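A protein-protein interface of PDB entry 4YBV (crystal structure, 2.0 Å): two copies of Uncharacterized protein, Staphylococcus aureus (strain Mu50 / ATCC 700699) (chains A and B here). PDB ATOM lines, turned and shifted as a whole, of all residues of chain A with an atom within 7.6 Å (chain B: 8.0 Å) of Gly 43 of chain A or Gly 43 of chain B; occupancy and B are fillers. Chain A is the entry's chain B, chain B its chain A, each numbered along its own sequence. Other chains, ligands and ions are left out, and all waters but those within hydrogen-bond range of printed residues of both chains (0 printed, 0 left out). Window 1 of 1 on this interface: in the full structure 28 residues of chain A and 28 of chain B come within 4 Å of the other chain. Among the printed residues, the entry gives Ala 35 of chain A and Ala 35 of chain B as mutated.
OE1 of Glu 50 of chain B is in hydrogen-bond range of NE2 of His 77 of chain A (2.8 Å). The side-chain carboxylate of Glu 50 of chain A lies within hydrogen-bond range of a ring nitrogen (NE2) of His 77 of chain B, 3.0 Å away. The side-chain hydroxyl (OG1) of Thr 51 of chain A is in hydrogen-bond range of a ring nitrogen (NE2) of His 41 of chain B, 2.9 Å away. The side-chain hydroxyl (OG1) of Thr 51 of chain B lies within hydrogen-bond range of a ring nitrogen (NE2) of His 41 of chain A, at 2.9 Å.
N of His 41 of chain B is in hydrogen-bond range of O of Val 33 of chain B, 2.8 Å away. The backbone carbonyl oxygen (O) of Ala 47 of chain B sits at hydrogen-bond distance from the side-chain hydroxyl (OG1) of Thr 51 of chain B (2.8 Å). N of His 41 of chain A is in hydrogen-bond range of O of Val 33 of chain A (2.9 Å). N of Gly 43 of chain A lies within hydrogen-bond range of ND1 of His 41 of chain A, at 2.8 Å. The backbone NH (N) of Gly 43 of chain B lies within hydrogen-bond range of a ring nitrogen (ND1) of His 41 of chain B, at 2.9 Å. The side-chain hydroxyl (OG1) of Thr 51 of chain A sits at hydrogen-bond distance from the backbone carbonyl oxygen (O) of Ala 47 of chain A (2.8 Å).
Among the printed residues, merely in contact across the chains: Leu 7 of chain A with Phe 11 of chain B (3.9 Å), Leu 7 of chain A with His 41 of chain B (3.6 Å), Phe 11 of chain A with Leu 7 of chain B (3.95 Å), Phe 11 of chain A with Phe 11 of chain B (3.5 Å), His 41 of chain A with Leu 7 of chain B (3.1 Å), His 41 of chain A with Ala 47 of chain B (3.6 Å), Gly 42 of chain A with Glu 50 of chain B (3.8 Å), Gly 43 of chain A with Gly 43 of chain B (3.7 Å), Gly 43 of chain A with Ala 47 of chain B (3.7 Å), Gly 43 of chain A with Glu 50 of chain B (3.8 Å), Ile 46 of chain A with Ile 46 of chain B (3.8 Å), Ile 46 of chain A with Glu 50 of chain B (3.9 Å), Ala 47 of chain A with His 41 of chain B (3.7 Å), Ala 47 of chain A with Gly 43 of chain B (3.8 Å), Glu 50 of chain A with Gly 42 of chain B (3.8 Å), Glu 50 of chain A with Gly 43 of chain B (3.7 Å), Glu 50 of chain A with Ile 46 of chain B (3.9 Å) and His 77 of chain A with Met 73 of chain B (3.9 Å).
Of the printed residues of chain B, Phe 11 of chain A touches Leu 7 (3.95 Å) and Phe 11 (3.5 Å). Gly 42 of chain A touches just one residue of chain B: Glu 50. Gly 43 of chain A touches just these residues of chain B: Gly 43 (3.7 Å), Ala 47 (3.7 Å) and Glu 50 (3.8 Å). No residue of chain B comes within 4 Å of Ala 44 of chain A. Printed residues of chain B within 4 Å of Ile 46 of chain A: Ile 46 and Glu 50. Gly 49 of chain A touches none of the printed residues of chain B. Gly 43 of chain B touches just these residues of chain A: Gly 43, Ala 47 and Glu 50. The nearest residue of chain B that does not touch Gly 43 of chain A is Ile 46 of chain B (5.0 Å). The nearest residue of chain A that does not touch Gly 43 of chain B is Ile 46 of chain A (5.0 Å). The nearest printed residue of chain B that does not touch Ile 46 of chain A is Met 73 of chain B (4.1 Å).
Hydrophobic or aromatic side chains of chain B within 4 Å of the printed part of chain A: Leu 7, Phe 11, His 41, Ile 46, Ala 47, Met 73 and His 77. Hydrophobic or aromatic side chains of chain A that line the printed part of chain B: Leu 7, Phe 11, His 41, Ile 46, Ala 47 and His 77.
Leu 7 of chain A touches Phe 11 of chain B, and with the chains exchanged Phe 11 of chain A touches Leu 7 of chain B. Gly 43 of chain B touches its own counterpart, Gly 43 of chain A. Ile 46 of chain B touches its own counterpart, Ile 46 of chain A. His 77 of chain A touches Met 73 of chain B, but with the chains exchanged Met 73 of chain A does not touch His 77 of chain B (4.0003 Å). Positions printed for both chains: 7, 11, 27, 33, 35, 40, 41, 42, 43, 44, 45, 46, 47, 48, 49, 50, 51, 73, 77 and 115.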
ATOM      1  N   LEU A   7     -37.830  19.321  10.139  1.00  0.00           N
ATOM      2  CA  LEU A   7     -36.966  20.517  10.243  1.00  0.00           C
ATOM      3  C   LEU A   7     -37.368  21.527   9.159  1.00  0.00           C
ATOM      4  O   LEU A   7     -37.358  22.756   9.382  1.00  0.00           O
ATOM      5  CB  LEU A   7     -35.461  20.165  10.111  1.00  0.00           C
ATOM      6  CG  LEU A   7     -34.562  21.390  10.362  1.00  0.00           C
ATOM      7  CD1 LEU A   7     -34.644  21.852  11.797  1.00  0.00           C
ATOM      8  CD2 LEU A   7     -33.098  21.164   9.985  1.00  0.00           C
ATOM      9  N   PHE A  11     -37.995  25.265  10.258  1.00  0.00           N
ATOM     10  CA  PHE A  11     -37.248  26.415   9.742  1.00  0.00           C
ATOM     11  C   PHE A  11     -38.069  27.206   8.703  1.00  0.00           C
ATOM     12  O   PHE A  11     -37.601  28.224   8.176  1.00  0.00           O
ATOM     13  CB  PHE A  11     -35.911  25.955   9.115  1.00  0.00           C
ATOM     14  CG  PHE A  11     -34.831  25.640  10.150  1.00  0.00           C
ATOM     15  CD1 PHE A  11     -35.158  25.608  11.505  1.00  0.00           C
ATOM     16  CD2 PHE A  11     -33.499  25.437   9.771  1.00  0.00           C
ATOM     17  CE1 PHE A  11     -34.174  25.342  12.491  1.00  0.00           C
ATOM     18  CE2 PHE A  11     -32.508  25.182  10.754  1.00  0.00           C
ATOM     19  CZ  PHE A  11     -32.854  25.137  12.101  1.00  0.00           C
ATOM     20  N   MET A  27     -35.817  30.787   3.416  1.00  0.00           N
ATOM     21  CA  MET A  27     -36.424  30.736   4.736  1.00  0.00           C
ATOM     22  C   MET A  27     -36.252  32.085   5.405  1.00  0.00           C
ATOM     23  O   MET A  27     -35.291  32.798   5.139  1.00  0.00           O
ATOM     24  CB  MET A  27     -35.817  29.613   5.594  1.00  0.00           C
ATOM     25  CG  MET A  27     -34.389  29.911   6.078  1.00  0.00           C
ATOM     26  SD  MET A  27     -33.691  28.500   6.971  1.00  0.00           S
ATOM     27  CE  MET A  27     -32.249  29.335   7.575  1.00  0.00           C
ATOM     28  N   VAL A  33     -34.126  30.831  14.717  1.00  0.00           N
ATOM     29  CA  VAL A  33     -32.961  30.321  13.995  1.00  0.00           C
ATOM     30  C   VAL A  33     -31.740  31.228  14.126  1.00  0.00           C
ATOM     31  O   VAL A  33     -30.761  31.090  13.382  1.00  0.00           O
ATOM     32  CB  VAL A  33     -33.249  30.122  12.498  1.00  0.00           C
ATOM     33  CG1 VAL A  33     -34.296  29.009  12.307  1.00  0.00           C
ATOM     34  CG2 VAL A  33     -33.685  31.455  11.874  1.00  0.00           C
ATOM     35  N   ALA A  35     -28.409  32.730  16.321  1.00  0.00           N
ATOM     36  CA  ALA A  35     -27.500  32.489  17.421  1.00  0.00           C
ATOM     37  C   ALA A  35     -27.833  33.526  18.488  1.00  0.00           C
ATOM     38  O   ALA A  35     -28.501  34.516  18.189  1.00  0.00           O
ATOM     39  CB  ALA A  35     -26.029  32.603  16.979  1.00  0.00           C
ATOM     40  N   LEU A  40     -28.490  35.259  12.131  1.00  0.00           N
ATOM     41  CA  LEU A  40     -28.788  33.895  11.706  1.00  0.00           C
ATOM     42  C   LEU A  40     -27.645  32.953  12.110  1.00  0.00           C
ATOM     43  O   LEU A  40     -26.481  33.220  11.847  1.00  0.00           O
ATOM     44  CB  LEU A  40     -29.038  33.825  10.183  1.00  0.00           C
ATOM     45  CG  LEU A  40     -29.257  32.431   9.600  1.00  0.00           C
ATOM     46  CD1 LEU A  40     -30.557  31.818  10.094  1.00  0.00           C
ATOM     47  CD2 LEU A  40     -29.207  32.502   8.017  1.00  0.00           C
ATOM     48  N   HIS A  41     -28.006  31.874  12.790  1.00  0.00           N
ATOM     49  CA  HIS A  41     -27.044  30.881  13.260  1.00  0.00           C
ATOM     50  C   HIS A  41     -26.391  30.195  12.072  1.00  0.00           C
ATOM     51  O   HIS A  41     -27.083  29.756  11.127  1.00  0.00           O
ATOM     52  CB  HIS A  41     -27.760  29.868  14.129  1.00  0.00           C
ATOM     53  CG  HIS A  41     -26.866  28.959  14.899  1.00  0.00           C
ATOM     54  ND1 HIS A  41     -26.160  27.931  14.314  1.00  0.00           N
ATOM     55  CD2 HIS A  41     -26.636  28.857  16.229  1.00  0.00           C
ATOM     56  CE1 HIS A  41     -25.508  27.261  15.245  1.00  0.00           C
ATOM     57  NE2 HIS A  41     -25.773  27.813  16.417  1.00  0.00           N
ATOM     58  N   GLY A  42     -25.069  30.121  12.082  1.00  0.00           N
ATOM     59  CA  GLY A  42     -24.362  29.497  10.971  1.00  0.00           C
ATOM     60  C   GLY A  42     -24.836  28.084  10.676  1.00  0.00           C
ATOM     61  O   GLY A  42     -24.917  27.665   9.537  1.00  0.00           O
ATOM     62  N   GLY A  43     -25.181  27.342  11.718  1.00  0.00           N
ATOM     63  CA  GLY A  43     -25.688  25.994  11.514  1.00  0.00           C
ATOM     64  C   GLY A  43     -27.046  25.903  10.782  1.00  0.00           C
ATOM     65  O   GLY A  43     -27.360  24.874  10.126  1.00  0.00           O
ATOM     66  N   ALA A  44     -27.888  26.929  10.969  1.00  0.00           N
ATOM     67  CA  ALA A  44     -29.202  26.990  10.335  1.00  0.00           C
ATOM     68  C   ALA A  44     -29.015  27.230   8.840  1.00  0.00           C
ATOM     69  O   ALA A  44     -29.728  26.664   7.987  1.00  0.00           O
ATOM     70  CB  ALA A  44     -30.060  28.114  10.968  1.00  0.00           C
ATOM     71  N   SER A  45     -28.067  28.103   8.517  1.00  0.00           N
ATOM     72  CA  SER A  45     -27.738  28.364   7.108  1.00  0.00           C
ATOM     73  C   SER A  45     -27.196  27.080   6.474  1.00  0.00           C
ATOM     74  O   SER A  45     -27.629  26.658   5.383  1.00  0.00           O
ATOM     75  CB  SER A  45     -26.739  29.526   7.026  1.00  0.00           C
ATOM     76  OG  SER A  45     -26.206  29.629   5.736  1.00  0.00           O
ATOM     77  N   ILE A  46     -26.307  26.382   7.198  1.00  0.00           N
ATOM     78  CA  ILE A  46     -25.822  25.110   6.654  1.00  0.00           C
ATOM     79  C   ILE A  46     -26.977  24.085   6.475  1.00  0.00           C
ATOM     80  O   ILE A  46     -27.027  23.362   5.471  1.00  0.00           O
ATOM     81  CB  ILE A  46     -24.706  24.548   7.543  1.00  0.00           C
ATOM     82  CG1 ILE A  46     -23.440  25.391   7.332  1.00  0.00           C
ATOM     83  CG2 ILE A  46     -24.387  23.134   7.163  1.00  0.00           C
ATOM     84  CD1 ILE A  46     -22.383  25.163   8.442  1.00  0.00           C
ATOM     85  N   ALA A  47     -27.903  24.021   7.423  1.00  0.00           N
ATOM     86  CA  ALA A  47     -29.065  23.120   7.297  1.00  0.00           C
ATOM     87  C   ALA A  47     -29.882  23.415   6.029  1.00  0.00           C
ATOM     88  O   ALA A  47     -30.263  22.506   5.282  1.00  0.00           O
ATOM     89  CB  ALA A  47     -29.960  23.232   8.499  1.00  0.00           C
ATOM     90  N   LEU A  48     -30.108  24.692   5.804  1.00  0.00           N
ATOM     91  CA  LEU A  48     -30.727  25.155   4.535  1.00  0.00           C
ATOM     92  C   LEU A  48     -29.988  24.607   3.316  1.00  0.00           C
ATOM     93  O   LEU A  48     -30.597  24.006   2.408  1.00  0.00           O
ATOM     94  CB  LEU A  48     -30.771  26.679   4.487  1.00  0.00           C
ATOM     95  CG  LEU A  48     -31.518  27.266   3.270  1.00  0.00           C
ATOM     96  CD1 LEU A  48     -32.970  26.743   3.320  1.00  0.00           C
ATOM     97  CD2 LEU A  48     -31.491  28.795   3.327  1.00  0.00           C
ATOM     98  N   GLY A  49     -28.661  24.734   3.319  1.00  0.00           N
ATOM     99  CA  GLY A  49     -27.911  24.205   2.189  1.00  0.00           C
ATOM    100  C   GLY A  49     -27.936  22.706   1.979  1.00  0.00           C
ATOM    101  O   GLY A  49     -28.004  22.240   0.817  1.00  0.00           O
ATOM    102  N   GLU A  50     -27.869  21.941   3.088  1.00  0.00           N
ATOM    103  CA  GLU A  50     -27.927  20.487   3.032  1.00  0.00           C
ATOM    104  C   GLU A  50     -29.277  20.058   2.436  1.00  0.00           C
ATOM    105  O   GLU A  50     -29.334  19.141   1.639  1.00  0.00           O
ATOM    106  CB  GLU A  50     -27.758  19.831   4.401  1.00  0.00           C
ATOM    107  CG  GLU A  50     -27.882  18.321   4.274  1.00  0.00           C
ATOM    108  CD  GLU A  50     -26.909  17.546   5.160  1.00  0.00           C
ATOM    109  OE1 GLU A  50     -26.130  18.211   5.881  1.00  0.00           O
ATOM    110  OE2 GLU A  50     -26.937  16.272   5.146  1.00  0.00           O
ATOM    111  N   THR A  51     -30.335  20.726   2.887  1.00  0.00           N
ATOM    112  CA  THR A  51     -31.691  20.501   2.390  1.00  0.00           C
ATOM    113  C   THR A  51     -31.743  20.750   0.885  1.00  0.00           C
ATOM    114  O   THR A  51     -32.266  19.943   0.134  1.00  0.00           O
ATOM    115  CB  THR A  51     -32.673  21.430   3.086  1.00  0.00           C
ATOM    116  OG1 THR A  51     -32.609  21.184   4.503  1.00  0.00           O
ATOM    117  CG2 THR A  51     -34.112  21.173   2.588  1.00  0.00           C
ATOM    118  N   MET A  73     -20.101  17.659   3.925  1.00  0.00           N
ATOM    119  CA  MET A  73     -20.565  19.043   3.723  1.00  0.00           C
ATOM    120  C   MET A  73     -19.495  19.973   4.208  1.00  0.00           C
ATOM    121  O   MET A  73     -18.874  19.712   5.257  1.00  0.00           O
ATOM    122  CB  MET A  73     -21.870  19.354   4.496  1.00  0.00           C
ATOM    123  CG  MET A  73     -23.076  18.463   4.150  1.00  0.00           C
ATOM    124  SD  MET A  73     -23.993  18.921   2.617  1.00  0.00           S
ATOM    125  CE  MET A  73     -24.420  17.266   2.043  1.00  0.00           C
ATOM    126  N   HIS A  77     -18.486  30.686   6.242  1.00  0.00           N
ATOM    127  CA  HIS A  77     -19.367  31.755   6.700  1.00  0.00           C
ATOM    128  C   HIS A  77     -18.768  33.095   6.308  1.00  0.00           C
ATOM    129  O   HIS A  77     -17.599  33.348   6.603  1.00  0.00           O
ATOM    130  CB  HIS A  77     -19.574  31.666   8.227  1.00  0.00           C
ATOM    131  CG  HIS A  77     -20.260  30.408   8.672  1.00  0.00           C
ATOM    132  ND1 HIS A  77     -21.447  29.984   8.118  1.00  0.00           N
ATOM    133  CD2 HIS A  77     -19.924  29.474   9.598  1.00  0.00           C
ATOM    134  CE1 HIS A  77     -21.836  28.866   8.714  1.00  0.00           C
ATOM    135  NE2 HIS A  77     -20.919  28.523   9.602  1.00  0.00           N
ATOM    136  N   THR A 115     -23.185  32.421   3.216  1.00  0.00           N
ATOM    137  CA  THR A 115     -22.472  31.141   3.325  1.00  0.00           C
ATOM    138  C   THR A 115     -22.178  30.586   1.934  1.00  0.00           C
ATOM    139  O   THR A 115     -23.018  30.670   1.040  1.00  0.00           O
ATOM    140  CB  THR A 115     -23.300  30.064   4.107  1.00  0.00           C
ATOM    141  OG1 THR A 115     -23.872  30.637   5.293  1.00  0.00           O
ATOM    142  CG2 THR A 115     -22.440  28.885   4.482  1.00  0.00           C
ATOM    143  N   LEU B   7     -31.829  29.576  18.563  1.00  0.00           N
ATOM    144  CA  LEU B   7     -31.699  28.226  18.027  1.00  0.00           C
ATOM    145  C   LEU B   7     -31.423  27.215  19.134  1.00  0.00           C
ATOM    146  O   LEU B   7     -32.041  26.152  19.186  1.00  0.00           O
ATOM    147  CB  LEU B   7     -30.587  28.171  16.978  1.00  0.00           C
ATOM    148  CG  LEU B   7     -30.337  26.811  16.323  1.00  0.00           C
ATOM    149  CD1 LEU B   7     -31.608  26.285  15.674  1.00  0.00           C
ATOM    150  CD2 LEU B   7     -29.209  26.901  15.308  1.00  0.00           C
ATOM    151  N   PHE B  11     -33.697  23.941  19.599  1.00  0.00           N
ATOM    152  CA  PHE B  11     -33.240  22.556  19.482  1.00  0.00           C
ATOM    153  C   PHE B  11     -33.195  21.873  20.848  1.00  0.00           C
ATOM    154  O   PHE B  11     -32.820  20.720  20.930  1.00  0.00           O
ATOM    155  CB  PHE B  11     -31.841  22.466  18.836  1.00  0.00           C
ATOM    156  CG  PHE B  11     -31.852  22.579  17.307  1.00  0.00           C
ATOM    157  CD1 PHE B  11     -33.035  22.864  16.627  1.00  0.00           C
ATOM    158  CD2 PHE B  11     -30.681  22.395  16.565  1.00  0.00           C
ATOM    159  CE1 PHE B  11     -33.042  22.959  15.218  1.00  0.00           C
ATOM    160  CE2 PHE B  11     -30.692  22.491  15.165  1.00  0.00           C
ATOM    161  CZ  PHE B  11     -31.871  22.769  14.502  1.00  0.00           C
ATOM    162  N   MET B  27     -28.762  17.142  22.680  1.00  0.00           N
ATOM    163  CA  MET B  27     -30.124  17.571  22.353  1.00  0.00           C
ATOM    164  C   MET B  27     -30.940  16.364  21.987  1.00  0.00           C
ATOM    165  O   MET B  27     -30.373  15.365  21.533  1.00  0.00           O
ATOM    166  CB  MET B  27     -30.116  18.606  21.205  1.00  0.00           C
ATOM    167  CG  MET B  27     -29.792  18.003  19.842  1.00  0.00           C
ATOM    168  SD  MET B  27     -29.641  19.264  18.518  1.00  0.00           S
ATOM    169  CE  MET B  27     -29.559  18.235  17.099  1.00  0.00           C
ATOM    170  N   VAL B  33     -36.506  18.272  14.455  1.00  0.00           N
ATOM    171  CA  VAL B  33     -35.143  18.335  13.902  1.00  0.00           C
ATOM    172  C   VAL B  33     -34.843  17.151  12.981  1.00  0.00           C
ATOM    173  O   VAL B  33     -33.688  16.929  12.588  1.00  0.00           O
ATOM    174  CB  VAL B  33     -34.065  18.390  15.040  1.00  0.00           C
ATOM    175  CG1 VAL B  33     -34.126  19.695  15.759  1.00  0.00           C
ATOM    176  CG2 VAL B  33     -34.254  17.254  16.027  1.00  0.00           C
ATOM    177  N   ALA B  35     -35.125  14.996   9.331  1.00  0.00           N
ATOM    178  CA  ALA B  35     -35.239  15.173   7.930  1.00  0.00           C
ATOM    179  C   ALA B  35     -36.613  14.497   7.717  1.00  0.00           C
ATOM    180  O   ALA B  35     -37.049  13.781   8.559  1.00  0.00           O
ATOM    181  CB  ALA B  35     -34.167  14.429   7.192  1.00  0.00           C
ATOM    182  N   LEU B  40     -32.498  12.160  12.286  1.00  0.00           N
ATOM    183  CA  LEU B  40     -32.076  13.503  12.602  1.00  0.00           C
ATOM    184  C   LEU B  40     -31.483  14.148  11.338  1.00  0.00           C
ATOM    185  O   LEU B  40     -30.667  13.551  10.668  1.00  0.00           O
ATOM    186  CB  LEU B  40     -31.042  13.497  13.726  1.00  0.00           C
ATOM    187  CG  LEU B  40     -30.446  14.827  14.171  1.00  0.00           C
ATOM    188  CD1 LEU B  40     -31.492  15.730  14.777  1.00  0.00           C
ATOM    189  CD2 LEU B  40     -29.253  14.565  15.133  1.00  0.00           C
ATOM    190  N   HIS B  41     -31.934  15.346  11.023  1.00  0.00           N
ATOM    191  CA  HIS B  41     -31.421  16.109   9.850  1.00  0.00           C
ATOM    192  C   HIS B  41     -29.908  16.368   9.988  1.00  0.00           C
ATOM    193  O   HIS B  41     -29.479  16.895  10.994  1.00  0.00           O
ATOM    194  CB  HIS B  41     -32.175  17.431   9.751  1.00  0.00           C
ATOM    195  CG  HIS B  41     -32.040  18.133   8.433  1.00  0.00           C
ATOM    196  ND1 HIS B  41     -30.867  18.739   8.028  1.00  0.00           N
ATOM    197  CD2 HIS B  41     -32.945  18.368   7.445  1.00  0.00           C
ATOM    198  CE1 HIS B  41     -31.054  19.305   6.850  1.00  0.00           C
ATOM    199  NE2 HIS B  41     -32.310  19.083   6.468  1.00  0.00           N
ATOM    200  N   GLY B  42     -29.106  16.014   8.992  1.00  0.00           N
ATOM    201  CA  GLY B  42     -27.668  16.287   9.056  1.00  0.00           C
ATOM    202  C   GLY B  42     -27.305  17.732   9.438  1.00  0.00           C
ATOM    203  O   GLY B  42     -26.283  18.031  10.117  1.00  0.00           O
ATOM    204  N   GLY B  43     -28.139  18.662   8.988  1.00  0.00           N
ATOM    205  CA  GLY B  43     -27.949  20.066   9.314  1.00  0.00           C
ATOM    206  C   GLY B  43     -28.113  20.418  10.788  1.00  0.00           C
ATOM    207  O   GLY B  43     -27.451  21.335  11.281  1.00  0.00           O
ATOM    208  N   ALA B  44     -29.040  19.730  11.464  1.00  0.00           N
ATOM    209  CA  ALA B  44     -29.295  19.909  12.885  1.00  0.00           C
ATOM    210  C   ALA B  44     -28.036  19.462  13.659  1.00  0.00           C
ATOM    211  O   ALA B  44     -27.567  20.161  14.548  1.00  0.00           O
ATOM    212  CB  ALA B  44     -30.552  19.095  13.325  1.00  0.00           C
ATOM    213  N   SER B  45     -27.528  18.286  13.299  1.00  0.00           N
ATOM    214  CA  SER B  45     -26.290  17.743  13.864  1.00  0.00           C
ATOM    215  C   SER B  45     -25.161  18.765  13.714  1.00  0.00           C
ATOM    216  O   SER B  45     -24.516  19.145  14.693  1.00  0.00           O
ATOM    217  CB  SER B  45     -25.919  16.433  13.167  1.00  0.00           C
ATOM    218  OG  SER B  45     -24.818  15.800  13.795  1.00  0.00           O
ATOM    219  N   ILE B  46     -24.964  19.248  12.479  1.00  0.00           N
ATOM    220  CA  ILE B  46     -23.927  20.240  12.218  1.00  0.00           C
ATOM    221  C   ILE B  46     -24.134  21.512  13.050  1.00  0.00           C
ATOM    222  O   ILE B  46     -23.165  22.047  13.612  1.00  0.00           O
ATOM    223  CB  ILE B  46     -23.846  20.632  10.700  1.00  0.00           C
ATOM    224  CG1 ILE B  46     -23.292  19.470   9.875  1.00  0.00           C
ATOM    225  CG2 ILE B  46     -22.952  21.877  10.499  1.00  0.00           C
ATOM    226  CD1 ILE B  46     -23.414  19.684   8.311  1.00  0.00           C
ATOM    227  N   ALA B  47     -25.385  21.963  13.185  1.00  0.00           N
ATOM    228  CA  ALA B  47     -25.675  23.178  13.968  1.00  0.00           C
ATOM    229  C   ALA B  47     -25.288  22.976  15.463  1.00  0.00           C
ATOM    230  O   ALA B  47     -24.729  23.878  16.103  1.00  0.00           O
ATOM    231  CB  ALA B  47     -27.139  23.536  13.870  1.00  0.00           C
ATOM    232  N   LEU B  48     -25.602  21.794  15.985  1.00  0.00           N
ATOM    233  CA  LEU B  48     -25.142  21.432  17.348  1.00  0.00           C
ATOM    234  C   LEU B  48     -23.611  21.536  17.444  1.00  0.00           C
ATOM    235  O   LEU B  48     -23.083  22.181  18.350  1.00  0.00           O
ATOM    236  CB  LEU B  48     -25.604  20.033  17.688  1.00  0.00           C
ATOM    237  CG  LEU B  48     -25.323  19.490  19.107  1.00  0.00           C
ATOM    238  CD1 LEU B  48     -26.136  20.246  20.143  1.00  0.00           C
ATOM    239  CD2 LEU B  48     -25.686  18.033  19.140  1.00  0.00           C
ATOM    240  N   GLY B  49     -22.899  20.940  16.483  1.00  0.00           N
ATOM    241  CA  GLY B  49     -21.436  21.068  16.437  1.00  0.00           C
ATOM    242  C   GLY B  49     -20.883  22.494  16.417  1.00  0.00           C
ATOM    243  O   GLY B  49     -19.941  22.864  17.183  1.00  0.00           O
ATOM    244  N   GLU B  50     -21.448  23.328  15.538  1.00  0.00           N
ATOM    245  CA  GLU B  50     -21.002  24.718  15.457  1.00  0.00           C
ATOM    246  C   GLU B  50     -21.272  25.449  16.773  1.00  0.00           C
ATOM    247  O   GLU B  50     -20.425  26.242  17.235  1.00  0.00           O
ATOM    248  CB  GLU B  50     -21.657  25.478  14.290  1.00  0.00           C
ATOM    249  CG  GLU B  50     -21.130  26.912  14.205  1.00  0.00           C
ATOM    250  CD  GLU B  50     -21.198  27.537  12.805  1.00  0.00           C
ATOM    251  OE1 GLU B  50     -21.463  26.829  11.812  1.00  0.00           O
ATOM    252  OE2 GLU B  50     -20.996  28.761  12.700  1.00  0.00           O
ATOM    253  N   THR B  51     -22.430  25.165  17.380  1.00  0.00           N
ATOM    254  CA  THR B  51     -22.736  25.718  18.709  1.00  0.00           C
ATOM    255  C   THR B  51     -21.645  25.309  19.719  1.00  0.00           C
ATOM    256  O   THR B  51     -21.160  26.133  20.497  1.00  0.00           O
ATOM    257  CB  THR B  51     -24.110  25.251  19.215  1.00  0.00           C
ATOM    258  OG1 THR B  51     -25.128  25.653  18.264  1.00  0.00           O
ATOM    259  CG2 THR B  51     -24.403  25.858  20.589  1.00  0.00           C
ATOM    260  N   MET B  73     -16.623  25.427   8.495  1.00  0.00           N
ATOM    261  CA  MET B  73     -17.122  24.228   9.167  1.00  0.00           C
ATOM    262  C   MET B  73     -17.133  23.109   8.167  1.00  0.00           C
ATOM    263  O   MET B  73     -17.536  23.321   7.014  1.00  0.00           O
ATOM    264  CB  MET B  73     -18.552  24.424   9.699  1.00  0.00           C
ATOM    265  CG  MET B  73     -18.711  25.542  10.716  1.00  0.00           C
ATOM    266  SD  MET B  73     -18.043  25.031  12.335  1.00  0.00           S
ATOM    267  CE  MET B  73     -17.508  26.635  12.934  1.00  0.00           C
ATOM    268  N   HIS B  77     -21.086  12.824   7.548  1.00  0.00           N
ATOM    269  CA  HIS B  77     -22.226  12.142   8.125  1.00  0.00           C
ATOM    270  C   HIS B  77     -21.951  10.632   8.082  1.00  0.00           C
ATOM    271  O   HIS B  77     -21.539  10.119   7.035  1.00  0.00           O
ATOM    272  CB  HIS B  77     -23.512  12.543   7.349  1.00  0.00           C
ATOM    273  CG  HIS B  77     -23.848  14.014   7.456  1.00  0.00           C
ATOM    274  ND1 HIS B  77     -24.055  14.645   8.668  1.00  0.00           N
ATOM    275  CD2 HIS B  77     -24.018  14.965   6.506  1.00  0.00           C
ATOM    276  CE1 HIS B  77     -24.360  15.910   8.456  1.00  0.00           C
ATOM    277  NE2 HIS B  77     -24.334  16.135   7.150  1.00  0.00           N
ATOM    278  N   THR B 115     -21.921  12.070  13.221  1.00  0.00           N
ATOM    279  CA  THR B 115     -21.265  13.144  12.445  1.00  0.00           C
ATOM    280  C   THR B 115     -19.887  13.396  13.000  1.00  0.00           C
ATOM    281  O   THR B 115     -19.730  13.469  14.213  1.00  0.00           O
ATOM    282  CB  THR B 115     -22.042  14.482  12.520  1.00  0.00           C
ATOM    283  OG1 THR B 115     -23.397  14.261  12.101  1.00  0.00           O
ATOM    284  CG2 THR B 115     -21.440  15.537  11.600  1.00  0.00           C
ATOM    285  N   MET B 117     -16.784  16.258  12.614  1.00  0.00           N
ATOM    286  CA  MET B 117     -16.634  17.580  12.131  1.00  0.00           C
ATOM    287  C   MET B 117     -15.410  18.328  12.533  1.00  0.00           C
ATOM    288  O   MET B 117     -14.874  18.095  13.582  1.00  0.00           O
ATOM    289  CB  MET B 117     -17.705  18.428  12.820  1.00  0.00           C
ATOM    290  CG  MET B 117     -19.042  18.601  12.213  1.00  0.00           C
ATOM    291  SD  MET B 117     -20.220  19.654  13.098  1.00  0.00           S
ATOM    292  CE  MET B 117     -19.701  21.294  12.788  1.00  0.00           C
